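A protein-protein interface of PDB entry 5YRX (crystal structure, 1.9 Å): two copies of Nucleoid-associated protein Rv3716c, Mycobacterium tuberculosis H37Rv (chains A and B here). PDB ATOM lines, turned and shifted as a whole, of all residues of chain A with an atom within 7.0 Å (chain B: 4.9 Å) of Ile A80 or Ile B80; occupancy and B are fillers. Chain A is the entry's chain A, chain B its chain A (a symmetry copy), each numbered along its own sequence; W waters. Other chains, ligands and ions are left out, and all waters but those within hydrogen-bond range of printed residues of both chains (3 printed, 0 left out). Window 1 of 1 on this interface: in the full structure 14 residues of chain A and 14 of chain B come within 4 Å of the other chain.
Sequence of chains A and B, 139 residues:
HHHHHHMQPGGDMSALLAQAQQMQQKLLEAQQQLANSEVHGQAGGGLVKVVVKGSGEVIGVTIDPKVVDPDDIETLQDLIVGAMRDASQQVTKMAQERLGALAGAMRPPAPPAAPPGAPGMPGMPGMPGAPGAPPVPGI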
ATOM      1  N   ALA A  43      18.559   0.235 -28.376  1.00  0.00           N
ATOM      2  CA  ALA A  43      18.211   1.143 -29.494  1.00  0.00           C
ATOM      3  C   ALA A  43      17.971   2.529 -29.044  1.00  0.00           C
ATOM      4  O   ALA A  43      17.517   2.856 -27.909  1.00  0.00           O
ATOM      5  CB  ALA A  43      17.028   0.623 -30.316  1.00  0.00           C
ATOM      6  N   VAL A  48      15.636   2.085 -25.351  1.00  0.00           N
ATOM      7  CA  VAL A  48      15.220   0.712 -25.019  1.00  0.00           C
ATOM      8  C   VAL A  48      16.472  -0.058 -24.896  1.00  0.00           C
ATOM      9  O   VAL A  48      17.400   0.053 -25.778  1.00  0.00           O
ATOM     10  CB  VAL A  48      14.213   0.070 -26.026  1.00  0.00           C
ATOM     11  CG1 VAL A  48      13.924  -1.321 -25.531  1.00  0.00           C
ATOM     12  CG2 VAL A  48      12.922   0.919 -26.130  1.00  0.00           C
ATOM     13  N   VAL A  50      17.894  -4.030 -23.759  1.00  0.00           N
ATOM     14  CA  VAL A  50      17.496  -5.402 -23.499  1.00  0.00           C
ATOM     15  C   VAL A  50      18.733  -6.229 -23.046  1.00  0.00           C
ATOM     16  O   VAL A  50      19.912  -5.858 -23.356  1.00  0.00           O
ATOM     17  CB  VAL A  50      16.805  -6.099 -24.676  1.00  0.00           C
ATOM     18  CG1 VAL A  50      15.594  -5.385 -25.171  1.00  0.00           C
ATOM     19  CG2 VAL A  50      17.759  -6.317 -25.824  1.00  0.00           C
ATOM     20  N   VAL A  58      15.263 -13.920 -23.721  1.00  0.00           N
ATOM     21  CA  VAL A  58      15.232 -12.531 -23.328  1.00  0.00           C
ATOM     22  C   VAL A  58      15.033 -12.514 -21.840  1.00  0.00           C
ATOM     23  O   VAL A  58      14.058 -13.033 -21.382  1.00  0.00           O
ATOM     24  CB  VAL A  58      14.075 -11.775 -24.008  1.00  0.00           C
ATOM     25  CG1 VAL A  58      13.841 -10.432 -23.383  1.00  0.00           C
ATOM     26  CG2 VAL A  58      14.320 -11.631 -25.492  1.00  0.00           C
ATOM     27  N   VAL A  61      13.983  -6.188 -20.096  1.00  0.00           N
ATOM     28  CA  VAL A  61      13.759  -5.146 -21.039  1.00  0.00           C
ATOM     29  C   VAL A  61      13.619  -3.893 -20.201  1.00  0.00           C
ATOM     30  O   VAL A  61      12.892  -3.968 -19.195  1.00  0.00           O
ATOM     31  CB  VAL A  61      12.436  -5.341 -21.838  1.00  0.00           C
ATOM     32  CG1 VAL A  61      12.202  -4.118 -22.717  1.00  0.00           C
ATOM     33  CG2 VAL A  61      12.559  -6.573 -22.779  1.00  0.00           C
ATOM     34  N   ILE A  63      12.753   0.241 -20.435  1.00  0.00           N
ATOM     35  CA  ILE A  63      12.263   1.191 -21.344  1.00  0.00           C
ATOM     36  C   ILE A  63      12.351   2.556 -20.652  1.00  0.00           C
ATOM     37  O   ILE A  63      11.793   2.756 -19.595  1.00  0.00           O
ATOM     38  CB  ILE A  63      10.828   0.821 -21.732  1.00  0.00           C
ATOM     39  CG1 ILE A  63      10.757  -0.489 -22.504  1.00  0.00           C
ATOM     40  CG2 ILE A  63      10.238   1.925 -22.593  1.00  0.00           C
ATOM     41  CD1 ILE A  63       9.381  -1.009 -22.512  1.00  0.00           C
ATOM     42  N   ILE A  73       2.971   4.874 -30.049  1.00  0.00           N
ATOM     43  CA  ILE A  73       3.355   3.482 -29.680  1.00  0.00           C
ATOM     44  C   ILE A  73       4.268   2.946 -30.724  1.00  0.00           C
ATOM     45  O   ILE A  73       5.103   2.088 -30.474  1.00  0.00           O
ATOM     46  CB  ILE A  73       2.092   2.650 -29.443  1.00  0.00           C
ATOM     47  CG1 ILE A  73       1.286   3.321 -28.277  1.00  0.00           C
ATOM     48  CG2 ILE A  73       2.458   1.254 -29.205  1.00  0.00           C
ATOM     49  CD1 ILE A  73      -0.109   2.752 -28.002  1.00  0.00           C
ATOM     50  N   GLU A  74       4.090   3.404 -31.958  1.00  0.00           N
ATOM     51  CA  GLU A  74       4.852   2.860 -33.082  1.00  0.00           C
ATOM     52  C   GLU A  74       6.358   2.945 -32.840  1.00  0.00           C
ATOM     53  O   GLU A  74       7.097   1.984 -33.056  1.00  0.00           O
ATOM     54  CB  GLU A  74       4.487   3.585 -34.378  1.00  0.00           C
ATOM     55  CG  GLU A  74       5.146   3.006 -35.620  1.00  0.00           C
ATOM     56  CD  GLU A  74       4.784   1.552 -35.847  1.00  0.00           C
ATOM     57  OE1 GLU A  74       3.749   1.104 -35.309  1.00  0.00           O
ATOM     58  OE2 GLU A  74       5.533   0.856 -36.564  1.00  0.00           O
ATOM     59  N   THR A  75       6.790   4.114 -32.390  1.00  0.00           N
ATOM     60  CA  THR A  75       8.198   4.421 -32.113  1.00  0.00           C
ATOM     61  C   THR A  75       8.768   3.498 -31.051  1.00  0.00           C
ATOM     62  O   THR A  75       9.847   2.912 -31.200  1.00  0.00           O
ATOM     63  CB  THR A  75       8.374   5.883 -31.696  1.00  0.00           C
ATOM     64  OG1 THR A  75       8.302   6.682 -32.903  1.00  0.00           O
ATOM     65  CG2 THR A  75       9.741   6.053 -31.074  1.00  0.00           C
ATOM     66  N   LEU A  76       7.986   3.328 -30.008  1.00  0.00           N
ATOM     67  CA  LEU A  76       8.322   2.378 -28.908  1.00  0.00           C
ATOM     68  C   LEU A  76       8.515   0.957 -29.448  1.00  0.00           C
ATOM     69  O   LEU A  76       9.525   0.309 -29.166  1.00  0.00           O
ATOM     70  CB  LEU A  76       7.221   2.446 -27.866  1.00  0.00           C
ATOM     71  CG  LEU A  76       7.336   1.425 -26.743  1.00  0.00           C
ATOM     72  CD1 LEU A  76       8.639   1.529 -25.975  1.00  0.00           C
ATOM     73  CD2 LEU A  76       6.190   1.490 -25.796  1.00  0.00           C
ATOM     74  N   GLN A  77       7.553   0.473 -30.223  1.00  0.00           N
ATOM     75  CA  GLN A  77       7.638  -0.826 -30.823  1.00  0.00           C
ATOM     76  C   GLN A  77       8.900  -0.973 -31.672  1.00  0.00           C
ATOM     77  O   GLN A  77       9.605  -1.936 -31.545  1.00  0.00           O
ATOM     78  CB  GLN A  77       6.396  -1.117 -31.683  1.00  0.00           C
ATOM     79  CG  GLN A  77       5.111  -1.169 -30.905  1.00  0.00           C
ATOM     80  CD  GLN A  77       3.873  -1.294 -31.780  1.00  0.00           C
ATOM     81  OE1 GLN A  77       3.932  -1.181 -32.998  1.00  0.00           O
ATOM     82  NE2 GLN A  77       2.789  -1.515 -31.158  1.00  0.00           N
ATOM     83  N   ASP A  78       9.137   0.004 -32.545  1.00  0.00           N
ATOM     84  CA  ASP A  78      10.339  -0.032 -33.373  1.00  0.00           C
ATOM     85  C   ASP A  78      11.665  -0.079 -32.545  1.00  0.00           C
ATOM     86  O   ASP A  78      12.598  -0.791 -32.917  1.00  0.00           O
ATOM     87  CB  ASP A  78      10.313   1.144 -34.276  1.00  0.00           C
ATOM     88  CG  ASP A  78       9.275   1.027 -35.405  1.00  0.00           C
ATOM     89  OD1 ASP A  78       8.783  -0.098 -35.686  1.00  0.00           O
ATOM     90  OD2 ASP A  78       8.962   2.062 -36.009  1.00  0.00           O
ATOM     91  N   LEU A  79      11.686   0.663 -31.449  1.00  0.00           N
ATOM     92  CA  LEU A  79      12.880   0.622 -30.588  1.00  0.00           C
ATOM     93  C   LEU A  79      13.104  -0.706 -29.895  1.00  0.00           C
ATOM     94  O   LEU A  79      14.268  -1.129 -29.689  1.00  0.00           O
ATOM     95  CB  LEU A  79      12.817   1.787 -29.574  1.00  0.00           C
ATOM     96  CG  LEU A  79      12.996   3.179 -30.087  1.00  0.00           C
ATOM     97  CD1 LEU A  79      12.618   4.268 -29.091  1.00  0.00           C
ATOM     98  CD2 LEU A  79      14.428   3.413 -30.527  1.00  0.00           C
ATOM     99  N   ILE A  80      12.006  -1.402 -29.553  1.00  0.00           N
ATOM    100  CA  ILE A  80      12.131  -2.700 -28.947  1.00  0.00           C
ATOM    101  C   ILE A  80      12.650  -3.679 -29.963  1.00  0.00           C
ATOM    102  O   ILE A  80      13.618  -4.453 -29.675  1.00  0.00           O
ATOM    103  CB  ILE A  80      10.802  -3.176 -28.335  1.00  0.00           C
ATOM    104  CG1 ILE A  80      10.376  -2.301 -27.164  1.00  0.00           C
ATOM    105  CG2 ILE A  80      10.968  -4.706 -27.999  1.00  0.00           C
ATOM    106  CD1 ILE A  80       8.865  -2.289 -26.836  1.00  0.00           C
ATOM    107  N   VAL A  81      12.098  -3.680 -31.162  1.00  0.00           N
ATOM    108  CA  VAL A  81      12.617  -4.547 -32.199  1.00  0.00           C
ATOM    109  C   VAL A  81      14.105  -4.222 -32.475  1.00  0.00           C
ATOM    110  O   VAL A  81      14.985  -5.171 -32.645  1.00  0.00           O
ATOM    111  CB  VAL A  81      11.806  -4.329 -33.553  1.00  0.00           C
ATOM    112  CG1 VAL A  81      12.456  -5.050 -34.732  1.00  0.00           C
ATOM    113  CG2 VAL A  81      10.374  -4.850 -33.363  1.00  0.00           C
ATOM    114  N   GLY A  82      14.407  -2.943 -32.608  1.00  0.00           N
ATOM    115  CA  GLY A  82      15.769  -2.457 -32.797  1.00  0.00           C
ATOM    116  C   GLY A  82      16.745  -2.929 -31.707  1.00  0.00           C
ATOM    117  O   GLY A  82      17.852  -3.383 -31.977  1.00  0.00           O
ATOM    118  N   ALA A  83      16.362  -2.837 -30.445  1.00  0.00           N
ATOM    119  CA  ALA A  83      17.183  -3.295 -29.345  1.00  0.00           C
ATOM    120  C   ALA A  83      17.365  -4.803 -29.375  1.00  0.00           C
ATOM    121  O   ALA A  83      18.522  -5.330 -29.067  1.00  0.00           O
ATOM    122  CB  ALA A  83      16.564  -2.793 -28.008  1.00  0.00           C
ATOM    123  N   MET A  84      16.326  -5.557 -29.753  1.00  0.00           N
ATOM    124  CA  MET A  84      16.456  -7.020 -29.944  1.00  0.00           C
ATOM    125  C   MET A  84      17.418  -7.356 -31.066  1.00  0.00           C
ATOM    126  O   MET A  84      18.310  -8.229 -30.913  1.00  0.00           O
ATOM    127  CB  MET A  84      15.080  -7.681 -30.139  1.00  0.00           C
ATOM    128  CG  MET A  84      14.194  -7.591 -28.905  1.00  0.00           C
ATOM    129  SD  MET A  84      14.814  -8.506 -27.485  1.00  0.00           S
ATOM    130  CE  MET A  84      13.328  -8.347 -26.517  1.00  0.00           C
ATOM    131  N   ARG A  85      17.339  -6.582 -32.137  1.00  0.00           N
ATOM    132  CA  ARG A  85      18.286  -6.747 -33.251  1.00  0.00           C
ATOM    133  C   ARG A  85      19.721  -6.490 -32.866  1.00  0.00           C
ATOM    134  O   ARG A  85      20.609  -7.278 -33.227  1.00  0.00           O
ATOM    135  CB  ARG A  85      17.827  -5.892 -34.439  1.00  0.00           C
ATOM    136  CG  ARG A  85      18.776  -5.955 -35.637  1.00  0.00           C
ATOM    137  CD  ARG A  85      18.278  -5.213 -36.886  1.00  0.00           C
ATOM    138  NE  ARG A  85      16.928  -4.643 -36.764  1.00  0.00           N
ATOM    139  CZ  ARG A  85      16.640  -3.338 -36.575  1.00  0.00           C
ATOM    140  NH1 ARG A  85      17.616  -2.411 -36.470  1.00  0.00           N
ATOM    141  NH2 ARG A  85      15.352  -2.952 -36.484  1.00  0.00           N
ATOM    142  N   ASP A  86      19.949  -5.408 -32.109  1.00  0.00           N
ATOM    143  CA  ASP A  86      21.227  -5.080 -31.549  1.00  0.00           C
ATOM    144  C   ASP A  86      21.801  -6.209 -30.718  1.00  0.00           C
ATOM    145  O   ASP A  86      23.018  -6.606 -30.859  1.00  0.00           O
ATOM    146  CB  ASP A  86      21.171  -3.688 -30.856  1.00  0.00           C
ATOM    147  CG  ASP A  86      22.550  -3.235 -30.357  1.00  0.00           C
ATOM    148  OD1 ASP A  86      23.464  -3.220 -31.218  1.00  0.00           O
ATOM    149  OD2 ASP A  86      22.755  -3.070 -29.133  1.00  0.00           O
ATOM    150  N   VAL B  48       0.505  -7.478 -25.039  1.00  0.00           N
ATOM    151  CA  VAL B  48       1.730  -7.401 -25.852  1.00  0.00           C
ATOM    152  C   VAL B  48       1.710  -8.602 -26.707  1.00  0.00           C
ATOM    153  O   VAL B  48       1.432  -9.755 -26.212  1.00  0.00           O
ATOM    154  CB  VAL B  48       3.054  -7.265 -25.033  1.00  0.00           C
ATOM    155  CG1 VAL B  48       4.183  -7.219 -26.027  1.00  0.00           C
ATOM    156  CG2 VAL B  48       3.023  -5.998 -24.144  1.00  0.00           C
ATOM    157  N   VAL B  61       6.483  -6.132 -32.866  1.00  0.00           N
ATOM    158  CA  VAL B  61       6.027  -6.084 -31.518  1.00  0.00           C
ATOM    159  C   VAL B  61       4.818  -5.176 -31.553  1.00  0.00           C
ATOM    160  O   VAL B  61       4.930  -4.115 -32.194  1.00  0.00           O
ATOM    161  CB  VAL B  61       7.077  -5.451 -30.557  1.00  0.00           C
ATOM    162  CG1 VAL B  61       6.458  -5.309 -29.170  1.00  0.00           C
ATOM    163  CG2 VAL B  61       8.309  -6.390 -30.421  1.00  0.00           C
ATOM    164  N   ILE B  63       1.933  -3.302 -29.090  1.00  0.00           N
ATOM    165  CA  ILE B  63       1.672  -3.050 -27.735  1.00  0.00           C
ATOM    166  C   ILE B  63       0.303  -2.364 -27.666  1.00  0.00           C
ATOM    167  O   ILE B  63       0.092  -1.332 -28.265  1.00  0.00           O
ATOM    168  CB  ILE B  63       2.795  -2.180 -27.161  1.00  0.00           C
ATOM    169  CG1 ILE B  63       4.135  -2.902 -27.143  1.00  0.00           C
ATOM    170  CG2 ILE B  63       2.443  -1.774 -25.740  1.00  0.00           C
ATOM    171  CD1 ILE B  63       5.236  -1.942 -26.972  1.00  0.00           C
ATOM    172  N   LEU B  76       4.648  -3.102 -18.297  1.00  0.00           N
ATOM    173  CA  LEU B  76       4.926  -3.136 -19.762  1.00  0.00           C
ATOM    174  C   LEU B  76       6.157  -3.997 -20.069  1.00  0.00           C
ATOM    175  O   LEU B  76       6.106  -4.885 -20.922  1.00  0.00           O
ATOM    176  CB  LEU B  76       5.093  -1.709 -20.249  1.00  0.00           C
ATOM    177  CG  LEU B  76       5.531  -1.573 -21.701  1.00  0.00           C
ATOM    178  CD1 LEU B  76       4.575  -2.233 -22.675  1.00  0.00           C
ATOM    179  CD2 LEU B  76       5.752  -0.156 -22.098  1.00  0.00           C
ATOM    180  N   GLN B  77       7.259  -3.736 -19.377  1.00  0.00           N
ATOM    181  CA  GLN B  77       8.461  -4.499 -19.542  1.00  0.00           C
ATOM    182  C   GLN B  77       8.221  -5.989 -19.301  1.00  0.00           C
ATOM    183  O   GLN B  77       8.625  -6.801 -20.086  1.00  0.00           O
ATOM    184  CB  GLN B  77       9.568  -3.991 -18.602  1.00  0.00           C
ATOM    185  CG  GLN B  77      10.004  -2.579 -18.875  1.00  0.00           C
ATOM    186  CD  GLN B  77      10.978  -2.030 -17.843  1.00  0.00           C
ATOM    187  OE1 GLN B  77      11.226  -2.636 -16.807  1.00  0.00           O
ATOM    188  NE2 GLN B  77      11.500  -0.911 -18.132  1.00  0.00           N
ATOM    189  N   ASP B  78       7.572  -6.304 -18.182  1.00  0.00           N
ATOM    190  CA  ASP B  78       7.264  -7.700 -17.886  1.00  0.00           C
ATOM    191  C   ASP B  78       6.401  -8.396 -18.990  1.00  0.00           C
ATOM    192  O   ASP B  78       6.640  -9.560 -19.313  1.00  0.00           O
ATOM    193  CB  ASP B  78       6.589  -7.755 -16.567  1.00  0.00           C
ATOM    194  CG  ASP B  78       7.536  -7.490 -15.383  1.00  0.00           C
ATOM    195  OD1 ASP B  78       8.781  -7.573 -15.550  1.00  0.00           O
ATOM    196  OD2 ASP B  78       7.026  -7.208 -14.290  1.00  0.00           O
ATOM    197  N   LEU B  79       5.452  -7.651 -19.534  1.00  0.00           N
ATOM    198  CA  LEU B  79       4.640  -8.222 -20.621  1.00  0.00           C
ATOM    199  C   LEU B  79       5.405  -8.479 -21.903  1.00  0.00           C
ATOM    200  O   LEU B  79       5.118  -9.462 -22.630  1.00  0.00           O
ATOM    201  CB  LEU B  79       3.410  -7.317 -20.867  1.00  0.00           C
ATOM    202  CG  LEU B  79       2.340  -7.282 -19.825  1.00  0.00           C
ATOM    203  CD1 LEU B  79       1.333  -6.153 -19.997  1.00  0.00           C
ATOM    204  CD2 LEU B  79       1.582  -8.595 -19.785  1.00  0.00           C
ATOM    205  N   ILE B  80       6.408  -7.630 -22.188  1.00  0.00           N
ATOM    206  CA  ILE B  80       7.224  -7.840 -23.353  1.00  0.00           C
ATOM    207  C   ILE B  80       8.079  -9.060 -23.154  1.00  0.00           C
ATOM    208  O   ILE B  80       8.150  -9.951 -24.060  1.00  0.00           O
ATOM    209  CB  ILE B  80       8.078  -6.603 -23.683  1.00  0.00           C
ATOM    210  CG1 ILE B  80       7.217  -5.415 -24.089  1.00  0.00           C
ATOM    211  CG2 ILE B  80       9.146  -7.049 -24.752  1.00  0.00           C
ATOM    212  CD1 ILE B  80       7.847  -4.017 -23.893  1.00  0.00           C
ATOM    213  N   VAL B  81       8.713  -9.192 -22.004  1.00  0.00           N
ATOM    214  CA  VAL B  81       9.482 -10.388 -21.733  1.00  0.00           C
ATOM    215  C   VAL B  81       8.572 -11.638 -21.801  1.00  0.00           C
ATOM    216  O   VAL B  81       8.968 -12.734 -22.389  1.00  0.00           O
ATOM    217  CB  VAL B  81      10.113 -10.316 -20.271  1.00  0.00           C
ATOM    218  CG1 VAL B  81      10.741 -11.643 -19.853  1.00  0.00           C
ATOM    219  CG2 VAL B  81      11.181  -9.215 -20.246  1.00  0.00           C
ATOM    220  N   GLY B  82       7.419 -11.554 -21.161  1.00  0.00           N
ATOM    221  CA  GLY B  82       6.412 -12.609 -21.184  1.00  0.00           C
ATOM    222  C   GLY B  82       5.990 -13.024 -22.603  1.00  0.00           C
ATOM    223  O   GLY B  82       5.901 -14.201 -22.938  1.00  0.00           O
ATOM    224  N   ALA B  83       5.719 -12.069 -23.476  1.00  0.00           N
ATOM    225  CA  ALA B  83       5.358 -12.347 -24.850  1.00  0.00           C
ATOM    226  C   ALA B  83       6.511 -12.976 -25.613  1.00  0.00           C
ATOM    227  O   ALA B  83       6.281 -13.935 -26.472  1.00  0.00           O
ATOM    228  CB  ALA B  83       4.845 -11.037 -25.513  1.00  0.00           C
ATOM    229  N   MET B  84       7.750 -12.544 -25.354  1.00  0.00           N
ATOM    230  CA  MET B  84       8.940 -13.196 -25.948  1.00  0.00           C
ATOM    231  C   MET B  84       9.085 -14.631 -25.483  1.00  0.00           C
ATOM    232  O   MET B  84       9.315 -15.556 -26.304  1.00  0.00           O
ATOM    233  CB  MET B  84      10.213 -12.370 -25.692  1.00  0.00           C
ATOM    234  CG  MET B  84      10.200 -11.018 -26.391  1.00  0.00           C
ATOM    235  SD  MET B  84      10.213 -11.118 -28.188  1.00  0.00           S
ATOM    236  CE  MET B  84      10.517  -9.383 -28.452  1.00  0.00           C
HETATM  237  O   HOH W   1      11.499 -13.919 -22.197  1.00  0.00           O
HETATM  238  O   HOH W   2       3.551  -4.148 -34.774  1.00  0.00           O
HETATM  239  O   HOH W   3      14.376  -4.104 -16.678  1.00  0.00           O
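The backbone NH of Ile B63 lies close to the side-chain amide nitrogen of Gln A77. The side-chain amide oxygen of Gln B77 sits close to the backbone carbonyl oxygen of Val A61 (3.2 Å). O of Val B61 lies close to OE1 of Gln A77. The backbone NH of Ile A63 lies close to the side-chain amide nitrogen of Gln B77, at 2.9 Å.
OE1 of Glu A74 sits close to OE1 of Gln A77 (3.3 Å).
Among the printed residues, pairs that only touch across the chains: Ile A80 with Ile B80 (3.6 Å), Met A84 with Met B84 (3.6 Å), Ile A73 with Ile B63 (3.6 Å), Ile A63 with Ile B80 (3.6 Å), Ile A80 with Ile B63 (3.6 Å), Ile A63 with Leu B76 (3.8 Å), Leu A76 with Ile B63 (3.8 Å), Val A58 with Val B81 (3.9 Å), Val A81 with Val B61 (3.9 Å), Val A61 with Val B81 (3.9 Å), Val A61 with Ile B80 (3.97 Å) and Ile A80 with Val B61 (3.97 Å).
Printed residues of chain A within 4 Å of Ile B63: Ile A73 (3.6 Å), Leu A76 (3.8 Å), Gln A77 (2.9 Å) and Ile A80 (3.6 Å). Printed residues of chain B within 4 Å of Leu A76: Ile B63. The nearest printed residue of chain A that does not touch Val B61 is Asp A78 (5.9 Å).
Printed residues of chain A that touch a printed residue of chain B: Val A58, Val A61, Ile A63, Ile A73, Leu A76, Gln A77, Ile A80, Val A81 and Met A84. Hydrophobic or aromatic side chains of chain A that line the printed part of chain B: Val A61, Ile A63, Ile A73, Leu A76, Ile A80, Val A81 and Met A84. Hydrophobic or aromatic side chains of chain B within 4 Å of the printed part of chain A: Val B61, Ile B63, Leu B76, Ile B80, Val B81 and Met B84. Among the printed residues, no Asp or Glu carboxylate lies within 4 Å of a Lys or Arg side-chain nitrogen of the other chain.
Val A61 touches Gln B77, and with the chains exchanged Gln A77 touches Val B61. Val A61 touches Ile B80, and with the chains exchanged Ile A80 touches Val B61. Val A61 touches Val B81, and with the chains exchanged Val A81 touches Val B61. Ile A63 touches Leu B76, and with the chains exchanged Leu A76 touches Ile B63. Positions printed for both chains: 48, 61, 63, 76, 77, 78, 79, 80, 81, 82, 83 and 84. Of the 16 pairs that touch across the chains among the printed residues, 14 have their exchanged pair printed and touching as well.
Water W1 bridges the backbone carbonyl oxygen (O) of Val B81 and the backbone carbonyl oxygen (O) of Val A58. Water W2 lies within hydrogen-bond range of O of Val B61 (2.9 Å) and OE1 of Gln A77 (3.5 Å). Water W3 lies within hydrogen-bond range of O of Val A61 (2.9 Å) and OE1 of Gln B77 (3.5 Å).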
